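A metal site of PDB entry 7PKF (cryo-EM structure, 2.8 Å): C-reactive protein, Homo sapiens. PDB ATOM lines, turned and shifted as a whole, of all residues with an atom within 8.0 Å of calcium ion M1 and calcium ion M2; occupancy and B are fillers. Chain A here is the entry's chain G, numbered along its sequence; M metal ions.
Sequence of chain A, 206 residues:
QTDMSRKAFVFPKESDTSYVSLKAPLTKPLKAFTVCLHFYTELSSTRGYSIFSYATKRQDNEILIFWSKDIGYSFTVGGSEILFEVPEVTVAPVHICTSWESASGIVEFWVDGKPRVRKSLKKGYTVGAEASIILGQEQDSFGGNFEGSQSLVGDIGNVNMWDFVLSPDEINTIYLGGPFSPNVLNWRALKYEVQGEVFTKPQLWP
OE1 of Gln 59 lies close to OD1 of Asp 60 (3.4 Å). The side-chain amide oxygen of Gln 59 sits at hydrogen-bond distance from the backbone NH of Asn 61 (3.2 Å). O of Asn 145 sits at hydrogen-bond distance from N of Asp 140 (3.5 Å). The backbone carbonyl oxygen of Gln 150 sits at hydrogen-bond distance from the backbone NH of Ser 50 (2.9 Å). The side-chain hydroxyl of Ser 53 sits at hydrogen-bond distance from the side-chain amide nitrogen of Gln 139 (3.0 Å). NE2 of Gln 139 lies close to N of Ala 55, at 3.1 Å.
Within 4 Å of calcium ion M1: Glu 138, Asp 140, Glu 147 and Gln 150.
Within 4 Å of calcium ion M2: Asp 60, Asn 61, Glu 138, Gln 139 and Asp 140. The nearest printed residue that does not touch calcium ion M2 is Leu 64 (5.1 Å).
Calcium ion M1 is bound by OE1 of Glu 138 (2.5 Å), OD2 of Asp 140 (2.5 Å), OE1 of Gln 150 (2.5 Å), OE1 of Glu 147 (2.5 Å) and OD1 of Asp 140 (2.7 Å).
Calcium ion M2 is bound by the side-chain carboxylate (OD2) of Asp 60, the side-chain carboxylate (OE1) of Glu 138, the side-chain amide oxygen (OD1) of Asn 61 and the side-chain carboxylate (OE2) of Glu 138. Calcium ion M2 has four donor atoms within binding distance. Slightly farther from calcium ion M2 lies the side-chain carboxylate (OD1) of Asp 140 (3.0 Å). Slightly farther from calcium ion M2 lies the backbone carbonyl oxygen (O) of Gln 139 (3.0 Å).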
ATOM      1  N   SER A  50      -0.703  18.865 -22.903  1.00  0.00           N
ATOM      2  CA  SER A  50      -0.294  20.156 -23.446  1.00  0.00           C
ATOM      3  C   SER A  50       1.209  20.376 -23.329  1.00  0.00           C
ATOM      4  O   SER A  50       1.773  20.345 -22.232  1.00  0.00           O
ATOM      5  CB  SER A  50      -1.032  21.279 -22.724  1.00  0.00           C
ATOM      6  OG  SER A  50      -0.767  22.532 -23.316  1.00  0.00           O
ATOM      7  N   SER A  53       0.775  26.053 -24.835  1.00  0.00           N
ATOM      8  CA  SER A  53      -0.565  26.597 -24.957  1.00  0.00           C
ATOM      9  C   SER A  53      -0.500  28.119 -25.105  1.00  0.00           C
ATOM     10  O   SER A  53      -0.009  28.810 -24.216  1.00  0.00           O
ATOM     11  CB  SER A  53      -1.422  26.222 -23.756  1.00  0.00           C
ATOM     12  OG  SER A  53      -2.666  26.885 -23.787  1.00  0.00           O
ATOM     13  N   TYR A  54      -0.984  28.618 -26.241  1.00  0.00           N
ATOM     14  CA  TYR A  54      -1.122  30.044 -26.514  1.00  0.00           C
ATOM     15  C   TYR A  54      -2.585  30.335 -26.813  1.00  0.00           C
ATOM     16  O   TYR A  54      -3.147  29.788 -27.766  1.00  0.00           O
ATOM     17  CB  TYR A  54      -0.220  30.399 -27.709  1.00  0.00           C
ATOM     18  CG  TYR A  54      -0.100  31.843 -28.131  1.00  0.00           C
ATOM     19  CD1 TYR A  54      -1.153  32.496 -28.750  1.00  0.00           C
ATOM     20  CD2 TYR A  54       1.096  32.521 -27.987  1.00  0.00           C
ATOM     21  CE1 TYR A  54      -1.030  33.792 -29.188  1.00  0.00           C
ATOM     22  CE2 TYR A  54       1.234  33.830 -28.414  1.00  0.00           C
ATOM     23  CZ  TYR A  54       0.169  34.459 -29.024  1.00  0.00           C
ATOM     24  OH  TYR A  54       0.290  35.756 -29.439  1.00  0.00           O
ATOM     25  N   ALA A  55      -3.197  31.196 -26.003  1.00  0.00           N
ATOM     26  CA  ALA A  55      -4.592  31.580 -26.163  1.00  0.00           C
ATOM     27  C   ALA A  55      -4.742  33.084 -26.329  1.00  0.00           C
ATOM     28  O   ALA A  55      -4.073  33.868 -25.650  1.00  0.00           O
ATOM     29  CB  ALA A  55      -5.428  31.126 -24.966  1.00  0.00           C
ATOM     30  N   GLN A  59      -9.892  33.088 -28.957  1.00  0.00           N
ATOM     31  CA  GLN A  59      -9.569  31.713 -29.360  1.00  0.00           C
ATOM     32  C   GLN A  59      -8.603  31.127 -28.336  1.00  0.00           C
ATOM     33  O   GLN A  59      -7.471  31.604 -28.215  1.00  0.00           O
ATOM     34  CB  GLN A  59      -8.954  31.711 -30.758  1.00  0.00           C
ATOM     35  CG  GLN A  59      -8.538  30.344 -31.264  1.00  0.00           C
ATOM     36  CD  GLN A  59      -9.668  29.343 -31.230  1.00  0.00           C
ATOM     37  OE1 GLN A  59      -9.803  28.560 -30.290  1.00  0.00           O
ATOM     38  NE2 GLN A  59     -10.508  29.363 -32.269  1.00  0.00           N
ATOM     39  N   ASP A  60      -9.067  30.114 -27.605  1.00  0.00           N
ATOM     40  CA  ASP A  60      -8.245  29.505 -26.567  1.00  0.00           C
ATOM     41  C   ASP A  60      -7.161  28.590 -27.118  1.00  0.00           C
ATOM     42  O   ASP A  60      -6.172  28.332 -26.434  1.00  0.00           O
ATOM     43  CB  ASP A  60      -9.133  28.718 -25.603  1.00  0.00           C
ATOM     44  CG  ASP A  60      -9.732  27.482 -26.245  1.00  0.00           C
ATOM     45  OD1 ASP A  60     -10.623  27.638 -27.098  1.00  0.00           O
ATOM     46  OD2 ASP A  60      -9.312  26.367 -25.902  1.00  0.00           O
ATOM     47  N   ASN A  61      -7.328  28.088 -28.346  1.00  0.00           N
ATOM     48  CA  ASN A  61      -6.283  27.303 -29.001  1.00  0.00           C
ATOM     49  C   ASN A  61      -5.693  28.110 -30.150  1.00  0.00           C
ATOM     50  O   ASN A  61      -5.794  27.701 -31.308  1.00  0.00           O
ATOM     51  CB  ASN A  61      -6.829  25.976 -29.507  1.00  0.00           C
ATOM     52  CG  ASN A  61      -7.163  25.017 -28.386  1.00  0.00           C
ATOM     53  OD1 ASN A  61      -7.013  25.341 -27.215  1.00  0.00           O
ATOM     54  ND2 ASN A  61      -7.597  23.811 -28.751  1.00  0.00           N
ATOM     55  N   GLU A  62      -5.093  29.252 -29.851  1.00  0.00           N
ATOM     56  CA  GLU A  62      -4.633  30.107 -30.931  1.00  0.00           C
ATOM     57  C   GLU A  62      -3.284  29.642 -31.483  1.00  0.00           C
ATOM     58  O   GLU A  62      -3.082  29.627 -32.699  1.00  0.00           O
ATOM     59  CB  GLU A  62      -4.549  31.556 -30.439  1.00  0.00           C
ATOM     60  CG  GLU A  62      -3.985  32.549 -31.428  1.00  0.00           C
ATOM     61  CD  GLU A  62      -5.047  33.094 -32.353  1.00  0.00           C
ATOM     62  OE1 GLU A  62      -6.201  33.247 -31.915  1.00  0.00           O
ATOM     63  OE2 GLU A  62      -4.739  33.355 -33.534  1.00  0.00           O
ATOM     64  N   LEU A  64      -1.468  25.985 -30.174  1.00  0.00           N
ATOM     65  CA  LEU A  64      -1.318  24.910 -29.200  1.00  0.00           C
ATOM     66  C   LEU A  64      -0.492  23.792 -29.813  1.00  0.00           C
ATOM     67  O   LEU A  64      -0.778  23.328 -30.916  1.00  0.00           O
ATOM     68  CB  LEU A  64      -2.685  24.390 -28.735  1.00  0.00           C
ATOM     69  CG  LEU A  64      -2.733  23.095 -27.925  1.00  0.00           C
ATOM     70  CD1 LEU A  64      -2.256  23.337 -26.495  1.00  0.00           C
ATOM     71  CD2 LEU A  64      -4.136  22.517 -27.912  1.00  0.00           C
ATOM     72  N   PHE A  66       0.257  19.982 -28.876  1.00  0.00           N
ATOM     73  CA  PHE A  66      -0.354  18.970 -28.021  1.00  0.00           C
ATOM     74  C   PHE A  66       0.085  17.593 -28.479  1.00  0.00           C
ATOM     75  O   PHE A  66      -0.056  17.241 -29.649  1.00  0.00           O
ATOM     76  CB  PHE A  66      -1.891  19.088 -28.076  1.00  0.00           C
ATOM     77  CG  PHE A  66      -2.600  18.344 -26.983  1.00  0.00           C
ATOM     78  CD1 PHE A  66      -2.990  18.985 -25.825  1.00  0.00           C
ATOM     79  CD2 PHE A  66      -2.909  17.005 -27.139  1.00  0.00           C
ATOM     80  CE1 PHE A  66      -3.660  18.303 -24.829  1.00  0.00           C
ATOM     81  CE2 PHE A  66      -3.579  16.322 -26.143  1.00  0.00           C
ATOM     82  CZ  PHE A  66      -3.952  16.975 -24.997  1.00  0.00           C
ATOM     83  N   THR A  76      -1.859  23.018 -33.834  1.00  0.00           N
ATOM     84  CA  THR A  76      -3.024  23.769 -34.266  1.00  0.00           C
ATOM     85  C   THR A  76      -2.763  25.272 -34.204  1.00  0.00           C
ATOM     86  O   THR A  76      -2.122  25.765 -33.272  1.00  0.00           O
ATOM     87  CB  THR A  76      -4.247  23.434 -33.422  1.00  0.00           C
ATOM     88  OG1 THR A  76      -5.348  24.274 -33.797  1.00  0.00           O
ATOM     89  CG2 THR A  76      -3.962  23.629 -31.946  1.00  0.00           C
ATOM     90  N   GLN A 137      -0.220  23.414 -18.693  1.00  0.00           N
ATOM     91  CA  GLN A 137      -1.666  23.267 -18.740  1.00  0.00           C
ATOM     92  C   GLN A 137      -2.155  23.578 -20.148  1.00  0.00           C
ATOM     93  O   GLN A 137      -1.479  24.238 -20.926  1.00  0.00           O
ATOM     94  CB  GLN A 137      -2.362  24.176 -17.712  1.00  0.00           C
ATOM     95  CG  GLN A 137      -1.900  23.960 -16.285  1.00  0.00           C
ATOM     96  CD  GLN A 137      -2.244  22.580 -15.781  1.00  0.00           C
ATOM     97  OE1 GLN A 137      -3.152  21.927 -16.288  1.00  0.00           O
ATOM     98  NE2 GLN A 137      -1.517  22.125 -14.765  1.00  0.00           N
ATOM     99  N   GLU A 138      -3.344  23.073 -20.444  1.00  0.00           N
ATOM    100  CA  GLU A 138      -4.094  23.475 -21.635  1.00  0.00           C
ATOM    101  C   GLU A 138      -5.254  24.340 -21.185  1.00  0.00           C
ATOM    102  O   GLU A 138      -6.087  23.906 -20.385  1.00  0.00           O
ATOM    103  CB  GLU A 138      -4.588  22.242 -22.401  1.00  0.00           C
ATOM    104  CG  GLU A 138      -4.642  22.439 -23.901  1.00  0.00           C
ATOM    105  CD  GLU A 138      -5.744  23.387 -24.322  1.00  0.00           C
ATOM    106  OE1 GLU A 138      -6.791  23.429 -23.638  1.00  0.00           O
ATOM    107  OE2 GLU A 138      -5.563  24.110 -25.317  1.00  0.00           O
ATOM    108  N   GLN A 139      -5.321  25.554 -21.716  1.00  0.00           N
ATOM    109  CA  GLN A 139      -6.270  26.550 -21.258  1.00  0.00           C
ATOM    110  C   GLN A 139      -7.428  26.663 -22.246  1.00  0.00           C
ATOM    111  O   GLN A 139      -7.211  26.735 -23.455  1.00  0.00           O
ATOM    112  CB  GLN A 139      -5.594  27.909 -21.060  1.00  0.00           C
ATOM    113  CG  GLN A 139      -5.313  28.681 -22.330  1.00  0.00           C
ATOM    114  CD  GLN A 139      -4.132  29.620 -22.194  1.00  0.00           C
ATOM    115  OE1 GLN A 139      -3.940  30.229 -21.139  1.00  0.00           O
ATOM    116  NE2 GLN A 139      -3.377  29.781 -23.256  1.00  0.00           N
ATOM    117  N   ASP A 140      -8.651  26.686 -21.714  1.00  0.00           N
ATOM    118  CA  ASP A 140      -9.858  26.712 -22.527  1.00  0.00           C
ATOM    119  C   ASP A 140     -10.617  28.021 -22.388  1.00  0.00           C
ATOM    120  O   ASP A 140     -11.525  28.278 -23.193  1.00  0.00           O
ATOM    121  CB  ASP A 140     -10.776  25.548 -22.134  1.00  0.00           C
ATOM    122  CG  ASP A 140     -10.153  24.192 -22.403  1.00  0.00           C
ATOM    123  OD1 ASP A 140     -10.305  23.678 -23.530  1.00  0.00           O
ATOM    124  OD2 ASP A 140      -9.511  23.642 -21.486  1.00  0.00           O
ATOM    125  N   SER A 141     -10.277  28.843 -21.413  1.00  0.00           N
ATOM    126  CA  SER A 141     -10.531  30.276 -21.437  1.00  0.00           C
ATOM    127  C   SER A 141      -9.194  31.014 -21.505  1.00  0.00           C
ATOM    128  O   SER A 141      -8.118  30.396 -21.553  1.00  0.00           O
ATOM    129  CB  SER A 141     -11.342  30.707 -20.215  1.00  0.00           C
ATOM    130  OG  SER A 141     -10.564  30.611 -19.034  1.00  0.00           O
ATOM    131  N   GLY A 144      -7.335  30.319 -18.077  1.00  0.00           N
ATOM    132  CA  GLY A 144      -7.804  29.362 -17.110  1.00  0.00           C
ATOM    133  C   GLY A 144      -8.655  28.262 -17.717  1.00  0.00           C
ATOM    134  O   GLY A 144      -8.634  28.039 -18.929  1.00  0.00           O
ATOM    135  N   ASN A 145      -9.394  27.586 -16.841  1.00  0.00           N
ATOM    136  CA  ASN A 145     -10.150  26.380 -17.181  1.00  0.00           C
ATOM    137  C   ASN A 145      -9.235  25.301 -17.751  1.00  0.00           C
ATOM    138  O   ASN A 145      -9.393  24.844 -18.891  1.00  0.00           O
ATOM    139  CB  ASN A 145     -11.289  26.715 -18.150  1.00  0.00           C
ATOM    140  CG  ASN A 145     -12.326  27.628 -17.540  1.00  0.00           C
ATOM    141  OD1 ASN A 145     -12.104  28.821 -17.382  1.00  0.00           O
ATOM    142  ND2 ASN A 145     -13.471  27.058 -17.185  1.00  0.00           N
ATOM    143  N   PHE A 146      -8.263  24.894 -16.932  1.00  0.00           N
ATOM    144  CA  PHE A 146      -7.398  23.773 -17.253  1.00  0.00           C
ATOM    145  C   PHE A 146      -8.088  22.455 -16.933  1.00  0.00           C
ATOM    146  O   PHE A 146      -8.964  22.391 -16.059  1.00  0.00           O
ATOM    147  CB  PHE A 146      -6.075  23.867 -16.501  1.00  0.00           C
ATOM    148  CG  PHE A 146      -5.547  25.266 -16.388  1.00  0.00           C
ATOM    149  CD1 PHE A 146      -5.246  26.000 -17.510  1.00  0.00           C
ATOM    150  CD2 PHE A 146      -5.338  25.842 -15.149  1.00  0.00           C
ATOM    151  CE1 PHE A 146      -4.754  27.288 -17.409  1.00  0.00           C
ATOM    152  CE2 PHE A 146      -4.842  27.119 -15.029  1.00  0.00           C
ATOM    153  CZ  PHE A 146      -4.554  27.844 -16.171  1.00  0.00           C
ATOM    154  N   GLU A 147      -7.687  21.398 -17.630  1.00  0.00           N
ATOM    155  CA  GLU A 147      -8.066  20.039 -17.298  1.00  0.00           C
ATOM    156  C   GLU A 147      -6.814  19.255 -16.887  1.00  0.00           C
ATOM    157  O   GLU A 147      -5.839  19.205 -17.641  1.00  0.00           O
ATOM    158  CB  GLU A 147      -8.753  19.347 -18.473  1.00  0.00           C
ATOM    159  CG  GLU A 147     -10.083  19.965 -18.853  1.00  0.00           C
ATOM    160  CD  GLU A 147     -10.444  19.731 -20.312  1.00  0.00           C
ATOM    161  OE1 GLU A 147      -9.812  20.362 -21.184  1.00  0.00           O
ATOM    162  OE2 GLU A 147     -11.348  18.908 -20.573  1.00  0.00           O
ATOM    163  N   GLY A 148      -6.866  18.655 -15.699  1.00  0.00           N
ATOM    164  CA  GLY A 148      -5.717  17.911 -15.201  1.00  0.00           C
ATOM    165  C   GLY A 148      -5.303  16.751 -16.095  1.00  0.00           C
ATOM    166  O   GLY A 148      -4.114  16.430 -16.175  1.00  0.00           O
ATOM    167  N   SER A 149      -6.256  16.122 -16.775  1.00  0.00           N
ATOM    168  CA  SER A 149      -5.942  15.089 -17.748  1.00  0.00           C
ATOM    169  C   SER A 149      -5.170  15.594 -18.954  1.00  0.00           C
ATOM    170  O   SER A 149      -4.650  14.783 -19.727  1.00  0.00           O
ATOM    171  CB  SER A 149      -7.235  14.419 -18.223  1.00  0.00           C
ATOM    172  OG  SER A 149      -8.124  15.357 -18.796  1.00  0.00           O
ATOM    173  N   GLN A 150      -5.079  16.914 -19.144  1.00  0.00           N
ATOM    174  CA  GLN A 150      -4.250  17.492 -20.191  1.00  0.00           C
ATOM    175  C   GLN A 150      -3.007  18.213 -19.664  1.00  0.00           C
ATOM    176  O   GLN A 150      -2.289  18.835 -20.468  1.00  0.00           O
ATOM    177  CB  GLN A 150      -5.078  18.466 -21.034  1.00  0.00           C
ATOM    178  CG  GLN A 150      -6.205  17.792 -21.797  1.00  0.00           C
ATOM    179  CD  GLN A 150      -6.799  18.682 -22.873  1.00  0.00           C
ATOM    180  OE1 GLN A 150      -6.780  19.901 -22.756  1.00  0.00           O
ATOM    181  NE2 GLN A 150      -7.322  18.069 -23.931  1.00  0.00           N
HETATM  182 CA    CA M   1      -8.489  21.788 -22.829  1.00  0.00          CA
HETATM  183 CA    CA M   2      -8.038  24.521 -25.283  1.00  0.00          CA
